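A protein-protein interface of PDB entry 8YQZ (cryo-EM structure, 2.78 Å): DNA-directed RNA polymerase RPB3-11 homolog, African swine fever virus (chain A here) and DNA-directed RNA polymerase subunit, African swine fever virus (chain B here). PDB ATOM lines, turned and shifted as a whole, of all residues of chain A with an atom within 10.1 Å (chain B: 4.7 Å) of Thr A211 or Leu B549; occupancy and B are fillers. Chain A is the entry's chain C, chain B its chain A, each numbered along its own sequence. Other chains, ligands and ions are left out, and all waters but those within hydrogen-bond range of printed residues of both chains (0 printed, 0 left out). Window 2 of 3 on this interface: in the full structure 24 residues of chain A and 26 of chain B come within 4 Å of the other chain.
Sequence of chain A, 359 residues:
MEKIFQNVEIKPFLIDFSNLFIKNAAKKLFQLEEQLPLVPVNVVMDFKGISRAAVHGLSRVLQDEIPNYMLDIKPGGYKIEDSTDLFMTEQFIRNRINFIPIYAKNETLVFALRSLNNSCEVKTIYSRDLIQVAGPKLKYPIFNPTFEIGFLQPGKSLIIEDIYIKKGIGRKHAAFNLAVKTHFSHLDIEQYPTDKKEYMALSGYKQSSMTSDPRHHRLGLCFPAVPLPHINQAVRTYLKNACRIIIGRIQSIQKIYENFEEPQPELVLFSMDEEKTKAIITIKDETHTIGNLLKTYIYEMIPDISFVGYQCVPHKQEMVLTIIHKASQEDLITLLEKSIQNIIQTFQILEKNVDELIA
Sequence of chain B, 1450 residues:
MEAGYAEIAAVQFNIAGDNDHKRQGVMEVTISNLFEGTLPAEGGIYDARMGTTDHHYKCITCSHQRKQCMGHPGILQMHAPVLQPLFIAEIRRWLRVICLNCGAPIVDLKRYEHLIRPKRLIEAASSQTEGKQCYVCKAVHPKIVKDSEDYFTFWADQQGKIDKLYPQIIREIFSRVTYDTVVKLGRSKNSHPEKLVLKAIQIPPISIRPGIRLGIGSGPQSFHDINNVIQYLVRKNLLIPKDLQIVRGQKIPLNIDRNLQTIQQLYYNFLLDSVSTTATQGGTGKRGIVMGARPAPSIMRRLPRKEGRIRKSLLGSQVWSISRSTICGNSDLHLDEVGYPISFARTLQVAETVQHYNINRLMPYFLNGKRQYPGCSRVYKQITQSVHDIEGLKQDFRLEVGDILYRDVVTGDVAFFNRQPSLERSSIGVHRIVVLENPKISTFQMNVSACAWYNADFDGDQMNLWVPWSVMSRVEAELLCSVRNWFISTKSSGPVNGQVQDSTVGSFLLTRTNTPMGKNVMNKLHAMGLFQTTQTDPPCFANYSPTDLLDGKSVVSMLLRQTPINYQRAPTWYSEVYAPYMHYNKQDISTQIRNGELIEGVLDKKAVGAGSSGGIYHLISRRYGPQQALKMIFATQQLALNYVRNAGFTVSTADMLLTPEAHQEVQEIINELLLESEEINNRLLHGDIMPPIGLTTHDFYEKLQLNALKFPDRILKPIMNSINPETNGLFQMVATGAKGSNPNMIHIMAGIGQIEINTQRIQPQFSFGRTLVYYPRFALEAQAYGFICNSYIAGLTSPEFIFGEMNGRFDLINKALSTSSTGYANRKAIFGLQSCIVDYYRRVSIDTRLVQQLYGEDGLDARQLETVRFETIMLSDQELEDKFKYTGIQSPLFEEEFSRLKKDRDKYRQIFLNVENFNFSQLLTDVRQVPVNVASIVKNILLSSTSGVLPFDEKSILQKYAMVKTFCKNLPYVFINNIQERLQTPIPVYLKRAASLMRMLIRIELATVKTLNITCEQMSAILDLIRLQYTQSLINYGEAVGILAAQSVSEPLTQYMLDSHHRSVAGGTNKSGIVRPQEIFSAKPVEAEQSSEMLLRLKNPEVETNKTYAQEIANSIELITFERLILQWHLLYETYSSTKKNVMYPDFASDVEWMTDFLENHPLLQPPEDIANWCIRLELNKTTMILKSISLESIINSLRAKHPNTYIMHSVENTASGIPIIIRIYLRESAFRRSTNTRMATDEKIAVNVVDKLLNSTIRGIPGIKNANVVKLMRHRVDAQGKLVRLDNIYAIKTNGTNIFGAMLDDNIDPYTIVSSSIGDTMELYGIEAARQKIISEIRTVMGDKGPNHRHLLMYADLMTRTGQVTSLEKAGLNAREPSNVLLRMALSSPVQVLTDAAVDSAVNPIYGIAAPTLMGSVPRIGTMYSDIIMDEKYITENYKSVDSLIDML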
ATOM      1  N   ARG A  52      24.563  32.824  11.007  1.00  0.00           N
ATOM      2  CA  ARG A  52      25.859  32.553  11.600  1.00  0.00           C
ATOM      3  C   ARG A  52      26.995  32.747  10.618  1.00  0.00           C
ATOM      4  O   ARG A  52      28.145  32.811  11.045  1.00  0.00           O
ATOM      5  CB  ARG A  52      25.918  31.146  12.178  1.00  0.00           C
ATOM      6  CG  ARG A  52      26.042  30.075  11.160  1.00  0.00           C
ATOM      7  CD  ARG A  52      25.984  28.728  11.805  1.00  0.00           C
ATOM      8  NE  ARG A  52      25.325  27.791  10.910  1.00  0.00           N
ATOM      9  CZ  ARG A  52      24.837  26.619  11.276  1.00  0.00           C
ATOM     10  NH1 ARG A  52      24.956  26.178  12.513  1.00  0.00           N
ATOM     11  NH2 ARG A  52      24.192  25.882  10.384  1.00  0.00           N
ATOM     12  N   ILE A 189      18.368  27.259  19.822  1.00  0.00           N
ATOM     13  CA  ILE A 189      18.352  25.805  19.742  1.00  0.00           C
ATOM     14  C   ILE A 189      18.426  25.275  21.165  1.00  0.00           C
ATOM     15  O   ILE A 189      19.278  25.709  21.946  1.00  0.00           O
ATOM     16  CB  ILE A 189      19.512  25.261  18.888  1.00  0.00           C
ATOM     17  CG1 ILE A 189      19.524  25.919  17.520  1.00  0.00           C
ATOM     18  CG2 ILE A 189      19.393  23.768  18.690  1.00  0.00           C
ATOM     19  CD1 ILE A 189      20.655  25.473  16.662  1.00  0.00           C
ATOM     20  N   TYR A 205      23.038  19.998  21.466  1.00  0.00           N
ATOM     21  CA  TYR A 205      21.937  20.623  20.758  1.00  0.00           C
ATOM     22  C   TYR A 205      20.906  19.585  20.338  1.00  0.00           C
ATOM     23  O   TYR A 205      21.238  18.447  20.012  1.00  0.00           O
ATOM     24  CB  TYR A 205      22.458  21.367  19.534  1.00  0.00           C
ATOM     25  CG  TYR A 205      23.160  22.652  19.867  1.00  0.00           C
ATOM     26  CD1 TYR A 205      22.480  23.696  20.459  1.00  0.00           C
ATOM     27  CD2 TYR A 205      24.496  22.823  19.589  1.00  0.00           C
ATOM     28  CE1 TYR A 205      23.106  24.860  20.764  1.00  0.00           C
ATOM     29  CE2 TYR A 205      25.131  23.986  19.890  1.00  0.00           C
ATOM     30  CZ  TYR A 205      24.428  25.005  20.480  1.00  0.00           C
ATOM     31  OH  TYR A 205      25.051  26.181  20.795  1.00  0.00           O
ATOM     32  N   LYS A 206      19.643  19.988  20.343  1.00  0.00           N
ATOM     33  CA  LYS A 206      18.545  19.077  20.060  1.00  0.00           C
ATOM     34  C   LYS A 206      18.207  18.977  18.581  1.00  0.00           C
ATOM     35  O   LYS A 206      17.306  18.218  18.222  1.00  0.00           O
ATOM     36  CB  LYS A 206      17.305  19.494  20.843  1.00  0.00           C
ATOM     37  CG  LYS A 206      17.358  19.079  22.284  1.00  0.00           C
ATOM     38  CD  LYS A 206      16.112  19.457  23.025  1.00  0.00           C
ATOM     39  CE  LYS A 206      16.183  18.970  24.449  1.00  0.00           C
ATOM     40  NZ  LYS A 206      15.000  19.387  25.233  1.00  0.00           N
ATOM     41  N   GLN A 207      18.901  19.710  17.721  1.00  0.00           N
ATOM     42  CA  GLN A 207      18.739  19.611  16.282  1.00  0.00           C
ATOM     43  C   GLN A 207      20.079  19.252  15.662  1.00  0.00           C
ATOM     44  O   GLN A 207      21.128  19.605  16.195  1.00  0.00           O
ATOM     45  CB  GLN A 207      18.224  20.916  15.686  1.00  0.00           C
ATOM     46  CG  GLN A 207      17.082  21.539  16.445  1.00  0.00           C
ATOM     47  CD  GLN A 207      16.605  22.828  15.815  1.00  0.00           C
ATOM     48  OE1 GLN A 207      16.917  23.119  14.669  1.00  0.00           O
ATOM     49  NE2 GLN A 207      15.873  23.623  16.578  1.00  0.00           N
ATOM     50  N   SER A 208      20.044  18.528  14.554  1.00  0.00           N
ATOM     51  CA  SER A 208      21.260  18.258  13.807  1.00  0.00           C
ATOM     52  C   SER A 208      21.748  19.527  13.128  1.00  0.00           C
ATOM     53  O   SER A 208      20.963  20.404  12.775  1.00  0.00           O
ATOM     54  CB  SER A 208      21.010  17.171  12.766  1.00  0.00           C
ATOM     55  OG  SER A 208      22.171  16.909  12.012  1.00  0.00           O
ATOM     56  N   SER A 209      23.062  19.635  12.955  1.00  0.00           N
ATOM     57  CA  SER A 209      23.583  20.786  12.238  1.00  0.00           C
ATOM     58  C   SER A 209      23.362  20.685  10.739  1.00  0.00           C
ATOM     59  O   SER A 209      23.618  21.657  10.030  1.00  0.00           O
ATOM     60  CB  SER A 209      25.063  20.994  12.549  1.00  0.00           C
ATOM     61  OG  SER A 209      25.806  19.811  12.417  1.00  0.00           O
ATOM     62  N   MET A 210      22.891  19.546  10.246  1.00  0.00           N
ATOM     63  CA  MET A 210      22.519  19.402   8.849  1.00  0.00           C
ATOM     64  C   MET A 210      21.109  19.877   8.543  1.00  0.00           C
ATOM     65  O   MET A 210      20.711  19.845   7.382  1.00  0.00           O
ATOM     66  CB  MET A 210      22.670  17.952   8.407  1.00  0.00           C
ATOM     67  CG  MET A 210      24.081  17.448   8.444  1.00  0.00           C
ATOM     68  SD  MET A 210      24.891  17.856   6.893  1.00  0.00           S
ATOM     69  CE  MET A 210      26.051  16.527   6.762  1.00  0.00           C
ATOM     70  N   THR A 211      20.343  20.297   9.540  1.00  0.00           N
ATOM     71  CA  THR A 211      19.004  20.815   9.312  1.00  0.00           C
ATOM     72  C   THR A 211      18.699  22.090  10.070  1.00  0.00           C
ATOM     73  O   THR A 211      17.755  22.788   9.691  1.00  0.00           O
ATOM     74  CB  THR A 211      17.937  19.769   9.677  1.00  0.00           C
ATOM     75  OG1 THR A 211      18.237  19.190  10.949  1.00  0.00           O
ATOM     76  CG2 THR A 211      17.870  18.681   8.653  1.00  0.00           C
ATOM     77  N   SER A 212      19.451  22.423  11.113  1.00  0.00           N
ATOM     78  CA  SER A 212      19.168  23.605  11.911  1.00  0.00           C
ATOM     79  C   SER A 212      19.648  24.858  11.202  1.00  0.00           C
ATOM     80  O   SER A 212      20.624  24.830  10.452  1.00  0.00           O
ATOM     81  CB  SER A 212      19.829  23.501  13.282  1.00  0.00           C
ATOM     82  OG  SER A 212      21.218  23.711  13.192  1.00  0.00           O
ATOM     83  N   ASP A 213      18.934  25.957  11.424  1.00  0.00           N
ATOM     84  CA  ASP A 213      19.288  27.271  10.891  1.00  0.00           C
ATOM     85  C   ASP A 213      19.135  28.322  11.982  1.00  0.00           C
ATOM     86  O   ASP A 213      18.145  29.059  12.015  1.00  0.00           O
ATOM     87  CB  ASP A 213      18.422  27.615   9.681  1.00  0.00           C
ATOM     88  CG  ASP A 213      18.884  28.860   8.983  1.00  0.00           C
ATOM     89  OD1 ASP A 213      20.093  29.150   9.038  1.00  0.00           O
ATOM     90  OD2 ASP A 213      18.043  29.556   8.381  1.00  0.00           O
ATOM     91  N   PRO A 214      20.097  28.413  12.898  1.00  0.00           N
ATOM     92  CA  PRO A 214      19.960  29.348  14.019  1.00  0.00           C
ATOM     93  C   PRO A 214      20.149  30.794  13.593  1.00  0.00           C
ATOM     94  O   PRO A 214      20.906  31.095  12.670  1.00  0.00           O
ATOM     95  CB  PRO A 214      21.060  28.899  14.977  1.00  0.00           C
ATOM     96  CG  PRO A 214      22.067  28.277  14.110  1.00  0.00           C
ATOM     97  CD  PRO A 214      21.365  27.672  12.951  1.00  0.00           C
ATOM     98  N   TYR A 299      22.082  32.417  -1.508  1.00  0.00           N
ATOM     99  CA  TYR A 299      21.057  31.412  -1.259  1.00  0.00           C
ATOM    100  C   TYR A 299      19.801  32.024  -0.647  1.00  0.00           C
ATOM    101  O   TYR A 299      18.687  31.572  -0.927  1.00  0.00           O
ATOM    102  CB  TYR A 299      21.635  30.321  -0.367  1.00  0.00           C
ATOM    103  CG  TYR A 299      20.708  29.179  -0.076  1.00  0.00           C
ATOM    104  CD1 TYR A 299      20.165  28.425  -1.097  1.00  0.00           C
ATOM    105  CD2 TYR A 299      20.401  28.835   1.223  1.00  0.00           C
ATOM    106  CE1 TYR A 299      19.329  27.382  -0.830  1.00  0.00           C
ATOM    107  CE2 TYR A 299      19.570  27.795   1.496  1.00  0.00           C
ATOM    108  CZ  TYR A 299      19.038  27.069   0.466  1.00  0.00           C
ATOM    109  OH  TYR A 299      18.207  26.024   0.742  1.00  0.00           O
ATOM    110  N   VAL B 521      18.980  12.846   7.544  1.00  0.00           N
ATOM    111  CA  VAL B 521      18.583  13.765   6.486  1.00  0.00           C
ATOM    112  C   VAL B 521      19.332  15.082   6.646  1.00  0.00           C
ATOM    113  O   VAL B 521      19.800  15.430   7.729  1.00  0.00           O
ATOM    114  CB  VAL B 521      17.058  14.026   6.478  1.00  0.00           C
ATOM    115  CG1 VAL B 521      16.314  12.808   6.001  1.00  0.00           C
ATOM    116  CG2 VAL B 521      16.572  14.449   7.841  1.00  0.00           C
ATOM    117  N   MET B 522      19.436  15.820   5.540  1.00  0.00           N
ATOM    118  CA  MET B 522      19.978  17.171   5.528  1.00  0.00           C
ATOM    119  C   MET B 522      19.087  18.050   4.672  1.00  0.00           C
ATOM    120  O   MET B 522      18.323  17.551   3.851  1.00  0.00           O
ATOM    121  CB  MET B 522      21.412  17.242   4.987  1.00  0.00           C
ATOM    122  CG  MET B 522      21.642  16.555   3.663  1.00  0.00           C
ATOM    123  SD  MET B 522      23.314  15.921   3.501  1.00  0.00           S
ATOM    124  CE  MET B 522      22.975  14.184   3.384  1.00  0.00           C
ATOM    125  N   ASN B 523      19.183  19.362   4.871  1.00  0.00           N
ATOM    126  CA  ASN B 523      18.396  20.296   4.084  1.00  0.00           C
ATOM    127  C   ASN B 523      19.110  20.616   2.769  1.00  0.00           C
ATOM    128  O   ASN B 523      20.193  20.112   2.481  1.00  0.00           O
ATOM    129  CB  ASN B 523      18.079  21.554   4.894  1.00  0.00           C
ATOM    130  CG  ASN B 523      19.309  22.287   5.377  1.00  0.00           C
ATOM    131  OD1 ASN B 523      20.423  21.975   5.003  1.00  0.00           O
ATOM    132  ND2 ASN B 523      19.103  23.264   6.234  1.00  0.00           N
ATOM    133  N   THR B 547      13.616  24.137   2.911  1.00  0.00           N
ATOM    134  CA  THR B 547      13.228  23.297   4.033  1.00  0.00           C
ATOM    135  C   THR B 547      13.011  21.839   3.649  1.00  0.00           C
ATOM    136  O   THR B 547      12.660  21.035   4.513  1.00  0.00           O
ATOM    137  CB  THR B 547      11.969  23.857   4.688  1.00  0.00           C
ATOM    138  OG1 THR B 547      11.000  24.161   3.679  1.00  0.00           O
ATOM    139  CG2 THR B 547      12.294  25.120   5.458  1.00  0.00           C
ATOM    140  N   ASP B 548      13.208  21.479   2.384  1.00  0.00           N
ATOM    141  CA  ASP B 548      13.091  20.091   1.960  1.00  0.00           C
ATOM    142  C   ASP B 548      14.245  19.284   2.533  1.00  0.00           C
ATOM    143  O   ASP B 548      15.354  19.799   2.684  1.00  0.00           O
ATOM    144  CB  ASP B 548      13.088  19.985   0.439  1.00  0.00           C
ATOM    145  CG  ASP B 548      11.758  20.351  -0.172  1.00  0.00           C
ATOM    146  OD1 ASP B 548      10.753  20.418   0.557  1.00  0.00           O
ATOM    147  OD2 ASP B 548      11.710  20.567  -1.396  1.00  0.00           O
ATOM    148  N   LEU B 549      13.984  18.023   2.851  1.00  0.00           N
ATOM    149  CA  LEU B 549      14.975  17.149   3.458  1.00  0.00           C
ATOM    150  C   LEU B 549      15.364  16.040   2.495  1.00  0.00           C
ATOM    151  O   LEU B 549      14.512  15.474   1.807  1.00  0.00           O
ATOM    152  CB  LEU B 549      14.446  16.547   4.754  1.00  0.00           C
ATOM    153  CG  LEU B 549      13.959  17.546   5.794  1.00  0.00           C
ATOM    154  CD1 LEU B 549      13.283  16.814   6.922  1.00  0.00           C
ATOM    155  CD2 LEU B 549      15.108  18.372   6.309  1.00  0.00           C
ATOM    156  N   LEU B 550      16.657  15.738   2.445  1.00  0.00           N
ATOM    157  CA  LEU B 550      17.210  14.738   1.546  1.00  0.00           C
ATOM    158  C   LEU B 550      17.944  13.687   2.357  1.00  0.00           C
ATOM    159  O   LEU B 550      18.749  14.023   3.223  1.00  0.00           O
ATOM    160  CB  LEU B 550      18.168  15.375   0.546  1.00  0.00           C
ATOM    161  CG  LEU B 550      17.604  16.221  -0.585  1.00  0.00           C
ATOM    162  CD1 LEU B 550      17.565  17.678  -0.188  1.00  0.00           C
ATOM    163  CD2 LEU B 550      18.450  16.034  -1.806  1.00  0.00           C
ATOM    164  N   ASP B 551      17.672  12.421   2.080  1.00  0.00           N
ATOM    165  CA  ASP B 551      18.390  11.359   2.759  1.00  0.00           C
ATOM    166  C   ASP B 551      19.776  11.191   2.151  1.00  0.00           C
ATOM    167  O   ASP B 551      20.059  11.649   1.048  1.00  0.00           O
ATOM    168  CB  ASP B 551      17.609  10.053   2.685  1.00  0.00           C
ATOM    169  CG  ASP B 551      16.958   9.846   1.340  1.00  0.00           C
ATOM    170  OD1 ASP B 551      16.212  10.748   0.891  1.00  0.00           O
ATOM    171  OD2 ASP B 551      17.189   8.784   0.724  1.00  0.00           O
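The side-chain hydroxyl (OG) of Ser A208 sits close to the backbone NH (N) of Met A210 (3.3 Å).
The backbone carbonyl oxygen (O) of Met B522 lies within hydrogen-bond range of the backbone NH (N) of Leu B550 (2.8 Å).
The backbone carbonyl oxygen of Ser A208 sits at hydrogen-bond distance from the side-chain hydroxyl of Thr A211.
Among the printed residues, pairs that only touch across the chains: Met A210 with Val B521 (3.9 Å), Met A210 with Met B522 (3.3 Å), Thr A211 with Val B521 (3.9 Å), Thr A211 with Asn B523 (3.7 Å) and Thr A211 with Leu B549 (3.6 Å).
Printed residues of chain B that touch a printed residue of chain A: Val B521, Met B522, Asn B523 and Leu B549.
Printed residues of chain A that touch a printed residue of chain B: Met A210 and Thr A211.
Hydrophobic or aromatic side chains of chain A that line the printed part of chain B: Met A210.
Among the printed residues, 6 pairs touch across the chains.
The backbone NH of Asn B523 sits at hydrogen-bond distance from the backbone carbonyl oxygen of Met A210, at 3.0 Å.
Of chain B, only Val B521, Asn B523 and Leu B549 come within 4 Å of Thr A211.
Leu B549 touches just one residue of chain A: Thr A211 (3.6 Å).
Of the printed residues of chain B, Met A210 touches Val B521 (3.9 Å), Met B522 (3.3 Å) and Asn B523 (3.0 Å).
Of the printed residues of chain A, Asn B523 touches Met A210 and Thr A211.
The nearest residue of chain B that does not touch Thr A211 is Met B522 (4.1 Å).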
